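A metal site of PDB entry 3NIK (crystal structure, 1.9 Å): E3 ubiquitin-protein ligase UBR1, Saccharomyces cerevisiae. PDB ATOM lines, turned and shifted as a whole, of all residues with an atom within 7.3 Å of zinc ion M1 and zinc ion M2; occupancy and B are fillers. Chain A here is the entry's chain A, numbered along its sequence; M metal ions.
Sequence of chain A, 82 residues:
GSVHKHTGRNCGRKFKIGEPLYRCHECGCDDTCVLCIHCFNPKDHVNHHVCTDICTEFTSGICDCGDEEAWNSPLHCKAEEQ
Within 4 Å of zinc ion M2: Cys 11, Cys 36, Cys 39 and Cys 63.
Along chain A the residues within 4 Å of zinc ion M2 span positions 11 to 63.
The nearest printed residue that does not touch zinc ion M2 is Cys 65 (4.2 Å).
The nearest printed residue that does not touch zinc ion M1 is Cys 11 (4.4 Å).
Zinc ion M2 is bound by the side-chain sulfur of Cys 63, the side-chain sulfur of Cys 36, the side-chain sulfur of Cys 11 and the side-chain sulfur of Cys 39.
Zinc ion M2 has four donor atoms within binding distance.
Zinc ion M1 is bound by a ring nitrogen (NE2) of His 6 (2.1 Å), the side-chain sulfur of Cys 39 (2.3 Å), the side-chain sulfur of Cys 77 (2.3 Å) and the side-chain sulfur of Cys 65 (2.3 Å).
Zinc ion M1 has four donor atoms within binding distance.
ND1 of His 6 lies within hydrogen-bond range of N of Cys 11.
SG of Cys 11 sits close to N of Arg 13, at 3.5 Å.
N of Cys 63 is in hydrogen-bond range of O of Arg 13 (2.9 Å).
The backbone NH (N) of His 38 sits close to the side-chain sulfur (SG) of Cys 36 (3.4 Å).
O of Cys 11 is in hydrogen-bond range of NH2 of Arg 9 (2.9 Å).
O of Cys 63 sits at hydrogen-bond distance from N of Gly 12 (3.0 Å).
A ring nitrogen (ND1) of His 6 lies within hydrogen-bond range of the backbone carbonyl oxygen (O) of Arg 9.
The backbone NH (N) of Ala 79 sits close to the side-chain sulfur (SG) of Cys 77, 3.5 Å away.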
ATOM      1  N   HIS A   4     -12.901  -6.514  20.459  1.00  0.00           N
ATOM      2  CA  HIS A   4     -13.923  -5.633  19.949  1.00  0.00           C
ATOM      3  C   HIS A   4     -13.635  -5.220  18.496  1.00  0.00           C
ATOM      4  O   HIS A   4     -12.521  -4.825  18.166  1.00  0.00           O
ATOM      5  CB  HIS A   4     -14.025  -4.403  20.842  1.00  0.00           C
ATOM      6  CG  HIS A   4     -15.332  -3.686  20.723  1.00  0.00           C
ATOM      7  ND1 HIS A   4     -15.527  -2.649  19.824  1.00  0.00           N
ATOM      8  CD2 HIS A   4     -16.507  -3.856  21.361  1.00  0.00           C
ATOM      9  CE1 HIS A   4     -16.765  -2.214  19.938  1.00  0.00           C
ATOM     10  NE2 HIS A   4     -17.386  -2.926  20.863  1.00  0.00           N
ATOM     11  N   LYS A   5     -14.645  -5.344  17.623  1.00  0.00           N
ATOM     12  CA  LYS A   5     -14.554  -4.784  16.264  1.00  0.00           C
ATOM     13  C   LYS A   5     -14.951  -3.321  16.327  1.00  0.00           C
ATOM     14  O   LYS A   5     -15.844  -2.953  17.087  1.00  0.00           O
ATOM     15  CB  LYS A   5     -15.529  -5.467  15.287  1.00  0.00           C
ATOM     16  CG  LYS A   5     -15.268  -6.924  14.984  1.00  0.00           C
ATOM     17  CD  LYS A   5     -16.448  -7.509  14.222  1.00  0.00           C
ATOM     18  CE  LYS A   5     -16.534  -9.028  14.350  1.00  0.00           C
ATOM     19  NZ  LYS A   5     -15.495  -9.752  13.576  1.00  0.00           N
ATOM     20  N   HIS A   6     -14.321  -2.493  15.500  1.00  0.00           N
ATOM     21  CA  HIS A   6     -14.719  -1.096  15.397  1.00  0.00           C
ATOM     22  C   HIS A   6     -15.191  -0.780  13.979  1.00  0.00           C
ATOM     23  O   HIS A   6     -14.855   0.259  13.414  1.00  0.00           O
ATOM     24  CB  HIS A   6     -13.551  -0.189  15.821  1.00  0.00           C
ATOM     25  CG  HIS A   6     -12.305  -0.391  15.015  1.00  0.00           C
ATOM     26  ND1 HIS A   6     -12.053   0.313  13.848  1.00  0.00           N
ATOM     27  CD2 HIS A   6     -11.237  -1.201  15.199  1.00  0.00           C
ATOM     28  CE1 HIS A   6     -10.885  -0.069  13.354  1.00  0.00           C
ATOM     29  NE2 HIS A   6     -10.383  -0.987  14.152  1.00  0.00           N
ATOM     30  N   ARG A   9     -15.661   2.786  11.719  1.00  0.00           N
ATOM     31  CA  ARG A   9     -14.971   3.893  12.374  1.00  0.00           C
ATOM     32  C   ARG A   9     -13.518   3.510  12.670  1.00  0.00           C
ATOM     33  O   ARG A   9     -13.085   2.403  12.367  1.00  0.00           O
ATOM     34  CB  ARG A   9     -15.686   4.306  13.674  1.00  0.00           C
ATOM     35  CG  ARG A   9     -15.891   3.170  14.674  1.00  0.00           C
ATOM     36  CD  ARG A   9     -16.093   3.680  16.110  1.00  0.00           C
ATOM     37  NE  ARG A   9     -14.826   4.010  16.779  1.00  0.00           N
ATOM     38  CZ  ARG A   9     -14.687   4.272  18.075  1.00  0.00           C
ATOM     39  NH1 ARG A   9     -15.739   4.251  18.908  1.00  0.00           N
ATOM     40  NH2 ARG A   9     -13.479   4.551  18.566  1.00  0.00           N
ATOM     41  N   ASN A  10     -12.782   4.451  13.243  1.00  0.00           N
ATOM     42  CA  ASN A  10     -11.398   4.226  13.662  1.00  0.00           C
ATOM     43  C   ASN A  10     -11.384   3.434  14.963  1.00  0.00           C
ATOM     44  O   ASN A  10     -12.392   3.379  15.675  1.00  0.00           O
ATOM     45  CB  ASN A  10     -10.693   5.557  13.899  1.00  0.00           C
ATOM     46  CG  ASN A  10     -11.293   6.298  15.071  1.00  0.00           C
ATOM     47  OD1 ASN A  10     -12.505   6.522  15.122  1.00  0.00           O
ATOM     48  ND2 ASN A  10     -10.464   6.641  16.061  1.00  0.00           N
ATOM     49  N   CYS A  11     -10.241   2.818  15.282  1.00  0.00           N
ATOM     50  CA  CYS A  11     -10.080   2.109  16.549  1.00  0.00           C
ATOM     51  C   CYS A  11      -9.979   3.126  17.688  1.00  0.00           C
ATOM     52  O   CYS A  11     -10.886   3.232  18.539  1.00  0.00           O
ATOM     53  CB  CYS A  11      -8.837   1.206  16.507  1.00  0.00           C
ATOM     54  SG  CYS A  11      -8.450   0.430  18.080  1.00  0.00           S
ATOM     55  N   GLY A  12      -8.890   3.886  17.701  1.00  0.00           N
ATOM     56  CA  GLY A  12      -8.683   4.953  18.684  1.00  0.00           C
ATOM     57  C   GLY A  12      -8.382   4.465  20.084  1.00  0.00           C
ATOM     58  O   GLY A  12      -8.443   5.238  21.046  1.00  0.00           O
ATOM     59  N   ARG A  13      -8.069   3.181  20.211  1.00  0.00           N
ATOM     60  CA  ARG A  13      -7.745   2.587  21.502  1.00  0.00           C
ATOM     61  C   ARG A  13      -6.497   3.205  22.123  1.00  0.00           C
ATOM     62  O   ARG A  13      -5.438   3.209  21.501  1.00  0.00           O
ATOM     63  CB  ARG A  13      -7.529   1.071  21.356  1.00  0.00           C
ATOM     64  CG  ARG A  13      -7.488   0.310  22.657  1.00  0.00           C
ATOM     65  CD  ARG A  13      -7.447  -1.195  22.359  1.00  0.00           C
ATOM     66  NE  ARG A  13      -7.053  -1.962  23.527  1.00  0.00           N
ATOM     67  CZ  ARG A  13      -5.795  -2.127  23.945  1.00  0.00           C
ATOM     68  NH1 ARG A  13      -4.782  -1.574  23.283  1.00  0.00           N
ATOM     69  NH2 ARG A  13      -5.562  -2.845  25.029  1.00  0.00           N
ATOM     70  N   PHE A  15      -3.313   2.995  24.247  1.00  0.00           N
ATOM     71  CA  PHE A  15      -2.432   1.879  24.573  1.00  0.00           C
ATOM     72  C   PHE A  15      -2.319   1.716  26.077  1.00  0.00           C
ATOM     73  O   PHE A  15      -2.408   2.704  26.817  1.00  0.00           O
ATOM     74  CB  PHE A  15      -1.039   2.041  23.955  1.00  0.00           C
ATOM     75  CG  PHE A  15      -1.039   1.987  22.464  1.00  0.00           C
ATOM     76  CD1 PHE A  15      -0.864   0.781  21.788  1.00  0.00           C
ATOM     77  CD2 PHE A  15      -1.242   3.145  21.721  1.00  0.00           C
ATOM     78  CE1 PHE A  15      -0.884   0.727  20.410  1.00  0.00           C
ATOM     79  CE2 PHE A  15      -1.271   3.105  20.323  1.00  0.00           C
ATOM     80  CZ  PHE A  15      -1.094   1.891  19.669  1.00  0.00           C
ATOM     81  N   VAL A  34       0.313   4.366  14.135  1.00  0.00           N
ATOM     82  CA  VAL A  34       0.515   3.145  14.923  1.00  0.00           C
ATOM     83  C   VAL A  34      -0.742   2.278  14.985  1.00  0.00           C
ATOM     84  O   VAL A  34      -1.867   2.771  14.813  1.00  0.00           O
ATOM     85  CB  VAL A  34       0.981   3.446  16.369  1.00  0.00           C
ATOM     86  CG1 VAL A  34       2.398   4.022  16.371  1.00  0.00           C
ATOM     87  CG2 VAL A  34       0.013   4.389  17.099  1.00  0.00           C
ATOM     88  N   LEU A  35      -0.535   0.987  15.234  1.00  0.00           N
ATOM     89  CA  LEU A  35      -1.600  -0.004  15.340  1.00  0.00           C
ATOM     90  C   LEU A  35      -1.471  -0.771  16.632  1.00  0.00           C
ATOM     91  O   LEU A  35      -0.355  -1.062  17.083  1.00  0.00           O
ATOM     92  CB  LEU A  35      -1.547  -0.986  14.156  1.00  0.00           C
ATOM     93  CG  LEU A  35      -1.805  -0.380  12.779  1.00  0.00           C
ATOM     94  CD1 LEU A  35      -1.405  -1.344  11.644  1.00  0.00           C
ATOM     95  CD2 LEU A  35      -3.271   0.032  12.623  1.00  0.00           C
ATOM     96  N   CYS A  36      -2.612  -1.052  17.252  1.00  0.00           N
ATOM     97  CA  CYS A  36      -2.643  -1.836  18.473  1.00  0.00           C
ATOM     98  C   CYS A  36      -2.694  -3.321  18.174  1.00  0.00           C
ATOM     99  O   CYS A  36      -2.843  -3.739  17.026  1.00  0.00           O
ATOM    100  CB  CYS A  36      -3.840  -1.437  19.358  1.00  0.00           C
ATOM    101  SG  CYS A  36      -5.430  -2.113  18.817  1.00  0.00           S
ATOM    102  N   ILE A  37      -2.606  -4.102  19.237  1.00  0.00           N
ATOM    103  CA  ILE A  37      -2.531  -5.559  19.137  1.00  0.00           C
ATOM    104  C   ILE A  37      -3.844  -6.188  18.688  1.00  0.00           C
ATOM    105  O   ILE A  37      -3.840  -7.275  18.088  1.00  0.00           O
ATOM    106  CB  ILE A  37      -2.031  -6.172  20.473  1.00  0.00           C
ATOM    107  CG1 ILE A  37      -3.084  -6.042  21.575  1.00  0.00           C
ATOM    108  CG2 ILE A  37      -0.738  -5.532  20.865  1.00  0.00           C
ATOM    109  CD1 ILE A  37      -2.516  -6.015  22.987  1.00  0.00           C
ATOM    110  N   HIS A  38      -4.955  -5.505  18.948  1.00  0.00           N
ATOM    111  CA  HIS A  38      -6.268  -5.957  18.481  1.00  0.00           C
ATOM    112  C   HIS A  38      -6.325  -5.895  16.962  1.00  0.00           C
ATOM    113  O   HIS A  38      -7.002  -6.703  16.332  1.00  0.00           O
ATOM    114  CB  HIS A  38      -7.407  -5.081  19.029  1.00  0.00           C
ATOM    115  CG  HIS A  38      -7.539  -5.082  20.516  1.00  0.00           C
ATOM    116  ND1 HIS A  38      -6.574  -5.573  21.368  1.00  0.00           N
ATOM    117  CD2 HIS A  38      -8.525  -4.615  21.314  1.00  0.00           C
ATOM    118  CE1 HIS A  38      -6.973  -5.424  22.623  1.00  0.00           C
ATOM    119  NE2 HIS A  38      -8.153  -4.849  22.615  1.00  0.00           N
ATOM    120  N   CYS A  39      -5.597  -4.934  16.381  1.00  0.00           N
ATOM    121  CA  CYS A  39      -5.797  -4.522  14.992  1.00  0.00           C
ATOM    122  C   CYS A  39      -4.724  -4.983  14.014  1.00  0.00           C
ATOM    123  O   CYS A  39      -5.027  -5.330  12.874  1.00  0.00           O
ATOM    124  CB  CYS A  39      -5.879  -2.989  14.943  1.00  0.00           C
ATOM    125  SG  CYS A  39      -7.415  -2.360  15.671  1.00  0.00           S
ATOM    126  N   PHE A  40      -3.474  -4.907  14.467  1.00  0.00           N
ATOM    127  CA  PHE A  40      -2.325  -5.182  13.603  1.00  0.00           C
ATOM    128  C   PHE A  40      -2.461  -6.565  13.001  1.00  0.00           C
ATOM    129  O   PHE A  40      -2.556  -7.544  13.734  1.00  0.00           O
ATOM    130  CB  PHE A  40      -1.034  -5.090  14.412  1.00  0.00           C
ATOM    131  CG  PHE A  40       0.204  -5.463  13.628  1.00  0.00           C
ATOM    132  CD1 PHE A  40       0.793  -4.546  12.769  1.00  0.00           C
ATOM    133  CD2 PHE A  40       0.768  -6.738  13.742  1.00  0.00           C
ATOM    134  CE1 PHE A  40       1.937  -4.877  12.047  1.00  0.00           C
ATOM    135  CE2 PHE A  40       1.921  -7.089  13.018  1.00  0.00           C
ATOM    136  CZ  PHE A  40       2.500  -6.174  12.173  1.00  0.00           C
ATOM    137  N   ILE A  62      -2.859   6.529  20.672  1.00  0.00           N
ATOM    138  CA  ILE A  62      -4.077   5.803  20.321  1.00  0.00           C
ATOM    139  C   ILE A  62      -3.903   5.121  18.977  1.00  0.00           C
ATOM    140  O   ILE A  62      -3.172   5.625  18.119  1.00  0.00           O
ATOM    141  CB  ILE A  62      -5.345   6.718  20.298  1.00  0.00           C
ATOM    142  CG1 ILE A  62      -5.119   7.956  19.424  1.00  0.00           C
ATOM    143  CG2 ILE A  62      -5.738   7.125  21.720  1.00  0.00           C
ATOM    144  CD1 ILE A  62      -5.712   7.864  18.076  1.00  0.00           C
ATOM    145  N   CYS A  63      -4.576   3.986  18.815  1.00  0.00           N
ATOM    146  CA  CYS A  63      -4.478   3.185  17.609  1.00  0.00           C
ATOM    147  C   CYS A  63      -5.122   3.907  16.424  1.00  0.00           C
ATOM    148  O   CYS A  63      -6.219   4.441  16.537  1.00  0.00           O
ATOM    149  CB  CYS A  63      -5.125   1.822  17.829  1.00  0.00           C
ATOM    150  SG  CYS A  63      -5.176   0.820  16.365  1.00  0.00           S
ATOM    151  N   ASP A  64      -4.432   3.906  15.283  1.00  0.00           N
ATOM    152  CA  ASP A  64      -4.898   4.581  14.059  1.00  0.00           C
ATOM    153  C   ASP A  64      -5.604   3.666  13.063  1.00  0.00           C
ATOM    154  O   ASP A  64      -5.978   4.102  11.976  1.00  0.00           O
ATOM    155  CB  ASP A  64      -3.726   5.311  13.356  1.00  0.00           C
ATOM    156  CG  ASP A  64      -3.117   6.378  14.221  1.00  0.00           C
ATOM    157  OD1 ASP A  64      -3.822   7.341  14.635  1.00  0.00           O
ATOM    158  OD2 ASP A  64      -1.902   6.257  14.504  1.00  0.00           O
ATOM    159  N   CYS A  65      -5.798   2.396  13.419  1.00  0.00           N
ATOM    160  CA  CYS A  65      -6.550   1.501  12.532  1.00  0.00           C
ATOM    161  C   CYS A  65      -7.914   2.118  12.205  1.00  0.00           C
ATOM    162  O   CYS A  65      -8.626   2.554  13.090  1.00  0.00           O
ATOM    163  CB  CYS A  65      -6.750   0.142  13.212  1.00  0.00           C
ATOM    164  SG  CYS A  65      -7.491  -1.097  12.104  1.00  0.00           S
ATOM    165  N   GLY A  66      -8.268   2.163  10.928  1.00  0.00           N
ATOM    166  CA  GLY A  66      -9.586   2.713  10.546  1.00  0.00           C
ATOM    167  C   GLY A  66      -9.628   4.219  10.346  1.00  0.00           C
ATOM    168  O   GLY A  66     -10.676   4.780  10.007  1.00  0.00           O
ATOM    169  N   LEU A  75      -5.850  -1.430   5.128  1.00  0.00           N
ATOM    170  CA  LEU A  75      -5.588  -2.366   6.222  1.00  0.00           C
ATOM    171  C   LEU A  75      -6.738  -3.341   6.410  1.00  0.00           C
ATOM    172  O   LEU A  75      -7.892  -3.009   6.160  1.00  0.00           O
ATOM    173  CB  LEU A  75      -5.351  -1.632   7.549  1.00  0.00           C
ATOM    174  CG  LEU A  75      -4.201  -0.624   7.667  1.00  0.00           C
ATOM    175  CD1 LEU A  75      -4.198  -0.018   9.049  1.00  0.00           C
ATOM    176  CD2 LEU A  75      -2.851  -1.258   7.374  1.00  0.00           C
ATOM    177  N   HIS A  76      -6.409  -4.548   6.857  1.00  0.00           N
ATOM    178  CA  HIS A  76      -7.409  -5.559   7.143  1.00  0.00           C
ATOM    179  C   HIS A  76      -7.369  -5.835   8.645  1.00  0.00           C
ATOM    180  O   HIS A  76      -6.669  -6.739   9.109  1.00  0.00           O
ATOM    181  CB  HIS A  76      -7.163  -6.797   6.295  1.00  0.00           C
ATOM    182  CG  HIS A  76      -7.160  -6.516   4.831  1.00  0.00           C
ATOM    183  ND1 HIS A  76      -6.027  -6.144   4.145  1.00  0.00           N
ATOM    184  CD2 HIS A  76      -8.166  -6.498   3.918  1.00  0.00           C
ATOM    185  CE1 HIS A  76      -6.326  -5.931   2.873  1.00  0.00           C
ATOM    186  NE2 HIS A  76      -7.622  -6.143   2.707  1.00  0.00           N
ATOM    187  N   CYS A  77      -8.114  -5.035   9.398  1.00  0.00           N
ATOM    188  CA  CYS A  77      -8.104  -5.094  10.849  1.00  0.00           C
ATOM    189  C   CYS A  77      -8.252  -6.536  11.313  1.00  0.00           C
ATOM    190  O   CYS A  77      -9.218  -7.204  10.946  1.00  0.00           O
ATOM    191  CB  CYS A  77      -9.262  -4.263  11.416  1.00  0.00           C
ATOM    192  SG  CYS A  77      -9.404  -4.318  13.205  1.00  0.00           S
ATOM    193  N   LYS A  78      -7.290  -6.986  12.122  1.00  0.00           N
ATOM    194  CA  LYS A  78      -7.289  -8.342  12.689  1.00  0.00           C
ATOM    195  C   LYS A  78      -8.573  -8.677  13.446  1.00  0.00           C
ATOM    196  O   LYS A  78      -9.048  -9.829  13.396  1.00  0.00           O
ATOM    197  CB  LYS A  78      -6.060  -8.568  13.586  1.00  0.00           C
ATOM    198  CG  LYS A  78      -5.786 -10.052  13.852  1.00  0.00           C
ATOM    199  CD  LYS A  78      -4.614 -10.304  14.770  1.00  0.00           C
ATOM    200  CE  LYS A  78      -4.431 -11.811  14.985  1.00  0.00           C
ATOM    201  NZ  LYS A  78      -3.145 -12.140  15.654  1.00  0.00           N
ATOM    202  N   ALA A  79      -9.134  -7.697  14.149  1.00  0.00           N
ATOM    203  CA  ALA A  79     -10.383  -7.901  14.909  1.00  0.00           C
ATOM    204  C   ALA A  79     -11.531  -8.378  14.026  1.00  0.00           C
ATOM    205  O   ALA A  79     -12.433  -9.079  14.497  1.00  0.00           O
ATOM    206  CB  ALA A  79     -10.776  -6.628  15.668  1.00  0.00           C
ATOM    207  N   GLU A  80     -11.512  -7.994  12.763  1.00  0.00           N
ATOM    208  CA  GLU A  80     -12.566  -8.364  11.831  1.00  0.00           C
ATOM    209  C   GLU A  80     -12.505  -9.833  11.408  1.00  0.00           C
ATOM    210  O   GLU A  80     -13.462 -10.367  10.863  1.00  0.00           O
ATOM    211  CB  GLU A  80     -12.523  -7.466  10.590  1.00  0.00           C
ATOM    212  CG  GLU A  80     -12.767  -5.965  10.864  1.00  0.00           C
ATOM    213  CD  GLU A  80     -14.235  -5.627  11.094  1.00  0.00           C
ATOM    214  OE1 GLU A  80     -15.117  -6.443  10.715  1.00  0.00           O
ATOM    215  OE2 GLU A  80     -14.505  -4.551  11.660  1.00  0.00           O
HETATM  216 ZN    ZN M   1      -8.674  -2.206  13.771  1.00  0.00          ZN
HETATM  217 ZN    ZN M   2      -6.551  -0.735  17.313  1.00  0.00          ZN
